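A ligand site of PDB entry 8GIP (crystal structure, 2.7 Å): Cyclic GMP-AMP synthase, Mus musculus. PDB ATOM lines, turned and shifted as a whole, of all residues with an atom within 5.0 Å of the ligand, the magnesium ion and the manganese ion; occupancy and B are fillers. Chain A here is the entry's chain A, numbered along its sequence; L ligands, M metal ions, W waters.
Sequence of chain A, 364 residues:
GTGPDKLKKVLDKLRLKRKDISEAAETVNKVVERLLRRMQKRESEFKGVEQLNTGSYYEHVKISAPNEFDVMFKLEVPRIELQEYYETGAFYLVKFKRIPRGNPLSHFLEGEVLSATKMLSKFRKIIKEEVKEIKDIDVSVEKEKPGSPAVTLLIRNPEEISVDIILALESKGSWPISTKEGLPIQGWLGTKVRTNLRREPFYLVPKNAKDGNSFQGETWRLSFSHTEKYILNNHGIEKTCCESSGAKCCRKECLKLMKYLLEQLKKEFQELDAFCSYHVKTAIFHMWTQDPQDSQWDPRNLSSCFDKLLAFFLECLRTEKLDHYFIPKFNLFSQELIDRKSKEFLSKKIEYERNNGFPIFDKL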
ATOM      1  N   GLY A  55      12.663  -9.046   4.774  1.00  0.00           N
ATOM      2  CA  GLY A  55      13.045  -9.942   5.840  1.00  0.00           C
ATOM      3  C   GLY A  55      11.870 -10.525   6.581  1.00  0.00           C
ATOM      4  O   GLY A  55      10.706 -10.340   6.227  1.00  0.00           O
ATOM      5  N   SER A  56      12.189 -11.255   7.652  1.00  0.00           N
ATOM      6  CA  SER A  56      11.196 -12.162   8.194  1.00  0.00           C
ATOM      7  C   SER A  56      10.030 -11.395   8.780  1.00  0.00           C
ATOM      8  O   SER A  56       8.869 -11.760   8.548  1.00  0.00           O
ATOM      9  CB  SER A  56      11.813 -13.109   9.225  1.00  0.00           C
ATOM     10  OG  SER A  56      12.446 -12.416  10.293  1.00  0.00           O
ATOM     11  N   GLU A  59       7.598 -10.663   6.216  1.00  0.00           N
ATOM     12  CA  GLU A  59       7.067 -11.865   5.594  1.00  0.00           C
ATOM     13  C   GLU A  59       6.176 -12.655   6.547  1.00  0.00           C
ATOM     14  O   GLU A  59       5.511 -13.603   6.107  1.00  0.00           O
ATOM     15  CB  GLU A  59       8.216 -12.736   5.125  1.00  0.00           C
ATOM     16  CG  GLU A  59       9.108 -12.084   4.089  1.00  0.00           C
ATOM     17  CD  GLU A  59      10.493 -12.748   3.977  1.00  0.00           C
ATOM     18  OE1 GLU A  59      10.914 -13.472   4.928  1.00  0.00           O
ATOM     19  OE2 GLU A  59      11.167 -12.539   2.938  1.00  0.00           O
ATOM     20  N   LYS A  62       9.055 -14.099  11.255  1.00  0.00           N
ATOM     21  CA  LYS A  62       9.868 -13.749  12.407  1.00  0.00           C
ATOM     22  C   LYS A  62       9.366 -14.495  13.628  1.00  0.00           C
ATOM     23  O   LYS A  62       8.177 -14.412  13.950  1.00  0.00           O
ATOM     24  CB  LYS A  62       9.817 -12.229  12.637  1.00  0.00           C
ATOM     25  CG  LYS A  62      10.642 -11.664  13.779  1.00  0.00           C
ATOM     26  CD  LYS A  62      12.103 -11.993  13.664  1.00  0.00           C
ATOM     27  CE  LYS A  62      12.816 -11.540  14.895  1.00  0.00           C
ATOM     28  NZ  LYS A  62      13.758 -12.529  15.493  1.00  0.00           N
ATOM     29  N   GLU A  68      14.241  -8.106  15.500  1.00  0.00           N
ATOM     30  CA  GLU A  68      15.165  -7.873  14.395  1.00  0.00           C
ATOM     31  C   GLU A  68      14.375  -7.518  13.153  1.00  0.00           C
ATOM     32  O   GLU A  68      13.557  -8.311  12.679  1.00  0.00           O
ATOM     33  CB  GLU A  68      16.044  -9.093  14.166  1.00  0.00           C
ATOM     34  CG  GLU A  68      17.338  -8.749  13.526  1.00  0.00           C
ATOM     35  CD  GLU A  68      17.261  -8.835  12.030  1.00  0.00           C
ATOM     36  OE1 GLU A  68      16.216  -9.298  11.507  1.00  0.00           O
ATOM     37  OE2 GLU A  68      18.223  -8.433  11.357  1.00  0.00           O
ATOM     38  N   ASP A  70      14.523  -5.697   9.094  1.00  0.00           N
ATOM     39  CA  ASP A  70      15.403  -5.445   7.957  1.00  0.00           C
ATOM     40  C   ASP A  70      14.782  -4.396   7.044  1.00  0.00           C
ATOM     41  O   ASP A  70      13.599  -4.509   6.696  1.00  0.00           O
ATOM     42  CB  ASP A  70      15.683  -6.723   7.183  1.00  0.00           C
ATOM     43  CG  ASP A  70      16.276  -7.801   8.064  1.00  0.00           C
ATOM     44  OD1 ASP A  70      17.471  -7.718   8.370  1.00  0.00           O
ATOM     45  OD2 ASP A  70      15.552  -8.733   8.456  1.00  0.00           O
ATOM     46  N   ASP A 164      18.575  -3.613  10.675  1.00  0.00           N
ATOM     47  CA  ASP A 164      19.579  -3.573   9.625  1.00  0.00           C
ATOM     48  C   ASP A 164      19.118  -2.568   8.581  1.00  0.00           C
ATOM     49  O   ASP A 164      18.131  -2.812   7.871  1.00  0.00           O
ATOM     50  CB  ASP A 164      19.767  -4.957   9.018  1.00  0.00           C
ATOM     51  CG  ASP A 164      20.598  -5.862   9.897  1.00  0.00           C
ATOM     52  OD1 ASP A 164      21.280  -5.342  10.810  1.00  0.00           O
ATOM     53  OD2 ASP A 164      20.597  -7.081   9.678  1.00  0.00           O
ATOM     54  N   ARG A 221      27.006  -7.428  -4.319  1.00  0.00           N
ATOM     55  CA  ARG A 221      26.308  -8.699  -4.322  1.00  0.00           C
ATOM     56  C   ARG A 221      24.845  -8.462  -4.686  1.00  0.00           C
ATOM     57  O   ARG A 221      24.245  -7.477  -4.233  1.00  0.00           O
ATOM     58  CB  ARG A 221      26.436  -9.380  -2.936  1.00  0.00           C
ATOM     59  CG  ARG A 221      25.758 -10.753  -2.803  1.00  0.00           C
ATOM     60  CD  ARG A 221      25.357 -11.044  -1.362  1.00  0.00           C
ATOM     61  NE  ARG A 221      23.918 -10.868  -1.179  1.00  0.00           N
ATOM     62  CZ  ARG A 221      23.363 -10.337  -0.092  1.00  0.00           C
ATOM     63  NH1 ARG A 221      24.088 -10.037   0.982  1.00  0.00           N
ATOM     64  NH2 ARG A 221      22.048 -10.077  -0.092  1.00  0.00           N
ATOM     65  N   PHE A 224      17.651 -10.171  -3.712  1.00  0.00           N
ATOM     66  CA  PHE A 224      16.296 -10.472  -4.168  1.00  0.00           C
ATOM     67  C   PHE A 224      15.322 -10.503  -3.002  1.00  0.00           C
ATOM     68  O   PHE A 224      14.317 -11.204  -3.072  1.00  0.00           O
ATOM     69  CB  PHE A 224      16.259 -11.797  -4.949  1.00  0.00           C
ATOM     70  CG  PHE A 224      16.997 -11.720  -6.264  1.00  0.00           C
ATOM     71  CD1 PHE A 224      16.438 -11.061  -7.350  1.00  0.00           C
ATOM     72  CD2 PHE A 224      18.278 -12.240  -6.380  1.00  0.00           C
ATOM     73  CE1 PHE A 224      17.114 -10.960  -8.547  1.00  0.00           C
ATOM     74  CE2 PHE A 224      18.978 -12.135  -7.573  1.00  0.00           C
ATOM     75  CZ  PHE A 224      18.401 -11.492  -8.664  1.00  0.00           C
ATOM     76  N   SER A 225      15.612  -9.744  -1.933  1.00  0.00           N
ATOM     77  CA  SER A 225      14.719  -9.747  -0.780  1.00  0.00           C
ATOM     78  C   SER A 225      13.331  -9.303  -1.159  1.00  0.00           C
ATOM     79  O   SER A 225      12.362  -9.707  -0.515  1.00  0.00           O
ATOM     80  CB  SER A 225      15.215  -8.850   0.339  1.00  0.00           C
ATOM     81  OG  SER A 225      16.540  -9.158   0.673  1.00  0.00           O
ATOM     82  N   GLU A 228      11.644 -12.329  -2.700  1.00  0.00           N
ATOM     83  CA  GLU A 228      11.404 -13.335  -1.661  1.00  0.00           C
ATOM     84  C   GLU A 228      10.213 -12.927  -0.783  1.00  0.00           C
ATOM     85  O   GLU A 228       9.408 -13.783  -0.386  1.00  0.00           O
ATOM     86  CB  GLU A 228      12.674 -13.509  -0.827  1.00  0.00           C
ATOM     87  CG  GLU A 228      13.920 -13.861  -1.641  1.00  0.00           C
ATOM     88  CD  GLU A 228      15.182 -13.678  -0.821  1.00  0.00           C
ATOM     89  OE1 GLU A 228      15.052 -13.315   0.377  1.00  0.00           O
ATOM     90  OE2 GLU A 228      16.299 -13.907  -1.341  1.00  0.00           O
ATOM     91  N   LYS A 259      13.602 -22.526  11.005  1.00  0.00           N
ATOM     92  CA  LYS A 259      14.342 -21.338  11.438  1.00  0.00           C
ATOM     93  C   LYS A 259      14.738 -21.475  12.900  1.00  0.00           C
ATOM     94  O   LYS A 259      15.837 -21.057  13.299  1.00  0.00           O
ATOM     95  CB  LYS A 259      13.495 -20.084  11.252  1.00  0.00           C
ATOM     96  CG  LYS A 259      13.524 -19.507   9.896  1.00  0.00           C
ATOM     97  CD  LYS A 259      12.414 -18.465   9.753  1.00  0.00           C
ATOM     98  CE  LYS A 259      12.644 -17.280  10.671  1.00  0.00           C
ATOM     99  NZ  LYS A 259      13.751 -16.448  10.125  1.00  0.00           N
ATOM    100  N   GLU A 263      18.285 -21.468  14.944  1.00  0.00           N
ATOM    101  CA  GLU A 263      18.576 -20.491  15.996  1.00  0.00           C
ATOM    102  C   GLU A 263      18.977 -21.167  17.300  1.00  0.00           C
ATOM    103  O   GLU A 263      19.996 -20.820  17.912  1.00  0.00           O
ATOM    104  CB  GLU A 263      17.367 -19.582  16.251  1.00  0.00           C
ATOM    105  CG  GLU A 263      17.105 -18.566  15.165  1.00  0.00           C
ATOM    106  CD  GLU A 263      16.051 -17.518  15.524  1.00  0.00           C
ATOM    107  OE1 GLU A 263      15.761 -17.320  16.723  1.00  0.00           O
ATOM    108  OE2 GLU A 263      15.517 -16.854  14.587  1.00  0.00           O
ATOM    109  N   CYS A 276      23.415 -19.549   8.543  1.00  0.00           N
ATOM    110  CA  CYS A 276      22.508 -18.459   8.830  1.00  0.00           C
ATOM    111  C   CYS A 276      21.122 -18.897   8.383  1.00  0.00           C
ATOM    112  O   CYS A 276      20.953 -19.949   7.770  1.00  0.00           O
ATOM    113  CB  CYS A 276      22.945 -17.163   8.143  1.00  0.00           C
ATOM    114  SG  CYS A 276      22.911 -17.200   6.352  1.00  0.00           S
ATOM    115  N   SER A 277      20.137 -18.066   8.689  1.00  0.00           N
ATOM    116  CA  SER A 277      18.770 -18.441   8.418  1.00  0.00           C
ATOM    117  C   SER A 277      18.485 -18.476   6.930  1.00  0.00           C
ATOM    118  O   SER A 277      17.603 -19.225   6.490  1.00  0.00           O
ATOM    119  CB  SER A 277      17.810 -17.493   9.133  1.00  0.00           C
ATOM    120  OG  SER A 277      17.927 -16.184   8.621  1.00  0.00           O
ATOM    121  N   TYR A 278      19.213 -17.677   6.143  1.00  0.00           N
ATOM    122  CA  TYR A 278      19.011 -17.656   4.703  1.00  0.00           C
ATOM    123  C   TYR A 278      19.292 -19.015   4.090  1.00  0.00           C
ATOM    124  O   TYR A 278      18.781 -19.355   3.016  1.00  0.00           O
ATOM    125  CB  TYR A 278      19.911 -16.591   4.058  1.00  0.00           C
ATOM    126  CG  TYR A 278      19.533 -16.319   2.623  1.00  0.00           C
ATOM    127  CD1 TYR A 278      18.324 -15.713   2.331  1.00  0.00           C
ATOM    128  CD2 TYR A 278      20.348 -16.698   1.571  1.00  0.00           C
ATOM    129  CE1 TYR A 278      17.935 -15.462   1.015  1.00  0.00           C
ATOM    130  CE2 TYR A 278      19.969 -16.473   0.244  1.00  0.00           C
ATOM    131  CZ  TYR A 278      18.755 -15.840  -0.018  1.00  0.00           C
ATOM    132  OH  TYR A 278      18.329 -15.562  -1.296  1.00  0.00           O
ATOM    133  N   LYS A 281      16.058 -20.594   4.569  1.00  0.00           N
ATOM    134  CA  LYS A 281      15.083 -19.942   3.695  1.00  0.00           C
ATOM    135  C   LYS A 281      15.248 -20.424   2.260  1.00  0.00           C
ATOM    136  O   LYS A 281      14.260 -20.637   1.547  1.00  0.00           O
ATOM    137  CB  LYS A 281      15.210 -18.423   3.765  1.00  0.00           C
ATOM    138  CG  LYS A 281      14.134 -17.625   3.041  1.00  0.00           C
ATOM    139  CD  LYS A 281      14.369 -16.129   3.240  1.00  0.00           C
ATOM    140  CE  LYS A 281      13.166 -15.298   2.847  1.00  0.00           C
ATOM    141  NZ  LYS A 281      13.499 -13.869   2.497  1.00  0.00           N
ATOM    142  N   HIS A 324      21.824 -21.204  -4.747  1.00  0.00           N
ATOM    143  CA  HIS A 324      21.035 -19.985  -4.635  1.00  0.00           C
ATOM    144  C   HIS A 324      19.760 -20.142  -5.453  1.00  0.00           C
ATOM    145  O   HIS A 324      19.787 -20.635  -6.593  1.00  0.00           O
ATOM    146  CB  HIS A 324      21.851 -18.789  -5.132  1.00  0.00           C
ATOM    147  CG  HIS A 324      21.361 -17.461  -4.630  1.00  0.00           C
ATOM    148  ND1 HIS A 324      20.150 -16.916  -4.989  1.00  0.00           N
ATOM    149  CD2 HIS A 324      21.958 -16.556  -3.827  1.00  0.00           C
ATOM    150  CE1 HIS A 324      19.998 -15.736  -4.407  1.00  0.00           C
ATOM    151  NE2 HIS A 324      21.084 -15.487  -3.692  1.00  0.00           N
HETATM  152  P1  LIG L   1      15.730 -13.710  10.649  1.00  0.00           P
HETATM  153  O1  LIG L   1      16.829 -14.697  10.854  1.00  0.00           O
HETATM  154  O2  LIG L   1      14.454 -13.904  11.481  1.00  0.00           O
HETATM  155  O3  LIG L   1      16.172 -12.250  10.860  1.00  0.00           O
HETATM  156  P2  LIG L   1      15.563 -13.045   7.743  1.00  0.00           P
HETATM  157  O4  LIG L   1      15.236 -13.834   6.551  1.00  0.00           O
HETATM  158  O5  LIG L   1      14.952 -11.646   7.857  1.00  0.00           O
HETATM  159  O6  LIG L   1      15.251 -13.758   9.130  1.00  0.00           O
HETATM  160  P3  LIG L   1      18.186 -11.778   7.880  1.00  0.00           P
HETATM  161  O7  LIG L   1      19.488 -12.364   8.271  1.00  0.00           O
HETATM  162  O8  LIG L   1      17.525 -10.731   8.770  1.00  0.00           O
HETATM  163  O9  LIG L   1      17.145 -12.921   7.801  1.00  0.00           O
HETATM  164  O10 LIG L   1      18.351 -11.225   6.408  1.00  0.00           O
HETATM  165  C1  LIG L   1      17.413 -10.285   5.845  1.00  0.00           C
HETATM  166  C2  LIG L   1      17.177 -10.624   4.388  1.00  0.00           C
HETATM  167  O11 LIG L   1      18.356 -10.300   3.603  1.00  0.00           O
HETATM  168  C3  LIG L   1      16.883 -12.080   4.066  1.00  0.00           C
HETATM  169  O12 LIG L   1      15.502 -12.390   4.198  1.00  0.00           O
HETATM  170  C4  LIG L   1      17.337 -12.185   2.611  1.00  0.00           C
HETATM  171  O13 LIG L   1      16.359 -11.661   1.716  1.00  0.00           O
HETATM  172  C5  LIG L   1      18.579 -11.290   2.605  1.00  0.00           C
HETATM  173  N1  LIG L   1      19.783 -12.046   2.941  1.00  0.00           N
HETATM  174  C6  LIG L   1      20.248 -12.381   4.192  1.00  0.00           C
HETATM  175  N2  LIG L   1      21.323 -13.119   4.187  1.00  0.00           N
HETATM  176  C7  LIG L   1      21.579 -13.311   2.831  1.00  0.00           C
HETATM  177  C8  LIG L   1      22.593 -14.007   2.145  1.00  0.00           C
HETATM  178  N3  LIG L   1      23.591 -14.663   2.754  1.00  0.00           N
HETATM  179  N4  LIG L   1      22.559 -13.999   0.796  1.00  0.00           N
HETATM  180  C9  LIG L   1      21.571 -13.346   0.184  1.00  0.00           C
HETATM  181  N5  LIG L   1      20.561 -12.653   0.714  1.00  0.00           N
HETATM  182  C10 LIG L   1      20.635 -12.663   2.053  1.00  0.00           C
HETATM  183 MG    MG M   1      15.725 -10.530   9.769  1.00  0.00          MG
HETATM  184 MN    MN M   2      19.230  -9.038   9.506  1.00  0.00          MN
HETATM  185  O   HOH W   1      13.902 -10.072  10.268  1.00  0.00           O
HETATM  186  O   HOH W   2      18.463 -11.856  -1.341  1.00  0.00           O
HETATM  187  O   HOH W   3      13.288 -14.877  13.575  1.00  0.00           O
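OE1 of Glu 228 lies within hydrogen-bond range of O13 of the ligand (2.5 Å).
OG of Ser 225 lies within hydrogen-bond range of O13 of the ligand (2.7 Å).
N of Ser 56 lies close to O5 of the ligand (2.8 Å).
The side-chain hydroxyl of Ser 56 sits at hydrogen-bond distance from an oxygen (O2) of the ligand (2.8 Å).
The side-chain hydroxyl (OG) of Ser 277 is in hydrogen-bond range of an oxygen (O1) of the ligand, at 2.9 Å.
The side-chain amino group (NZ) of Lys 259 lies within salt-bridge range of an oxygen (O2) of the ligand (3.0 Å).
An oxygen (O12) of the ligand lies within hydrogen-bond range of the side-chain amino group (NZ) of Lys 281 (3.0 Å).
NH2 of Arg 221 is in hydrogen-bond range of N5 of the ligand (3.1 Å).
Water W1 lies within hydrogen-bond range of OG of Ser 56 (2.8 Å) and O of Glu 68 (3.0 Å).
Water W3 lies within hydrogen-bond range of an oxygen (O2) of the ligand (2.6 Å), the side-chain amino group of Lys 62 (3.1 Å) and the side-chain carboxylate of Glu 263 (3.1 Å).
Water W2 lies within hydrogen-bond range of the side-chain carboxylate of Glu 228 (3.0 Å), the backbone NH of Phe 224 (3.0 Å) and a nitrogen (N5) of the ligand (3.0 Å).
OG of Ser 56 touches the magnesium ion, at 3.8 Å.
Three residues have an atom within 4 Å of the magnesium ion: Ser 56, Glu 68 and Asp 70.
Within 4 Å of the manganese ion: Glu 68, Asp 70 and Asp 164.
The side-chain amino group (NZ) of Lys 281 is in salt-bridge range of the side-chain carboxylate (OE1) of Glu 228 (2.7 Å).
OH of Tyr 278 is in hydrogen-bond range of OE2 of Glu 228 (2.6 Å).
The side-chain amino group (NZ) of Lys 281 is in salt-bridge range of the side-chain carboxylate (OE2) of Glu 59 (2.7 Å).
The side-chain sulfur of Cys 276 lies close to the backbone NH of Tyr 278, at 3.7 Å.
Water W1 binds the magnesium ion (1.9 Å).
O8 of the ligand binds the magnesium ion (2.1 Å).
O3 of the ligand is bound to the magnesium ion.
OE1 of Glu 68 is bound to the magnesium ion, at 2.2 Å.
OD2 of Asp 70 is bound to the magnesium ion (2.2 Å).
O5 of the ligand binds the magnesium ion, at 2.3 Å.
The manganese ion is bound by OE2 of Glu 68 (2.2 Å), OD2 of Asp 164 (2.4 Å), OD1 of Asp 70 (2.5 Å) and O8 of the ligand (2.5 Å).
The manganese ion has four donor atoms within binding distance.
CA of Gly 55 touches O5 of the ligand, at 3.3 Å.
Lys 62 touches the ligand (CD to O2, 3.7 Å).
Tyr 278 touches the ligand (CE2 to C9, 3.5 Å).
Hydrophobic or aromatic side chains within 4 Å of the ligand: Tyr 278.
Of the 18 residues printed, 12 come within 4 Å of the ligand.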
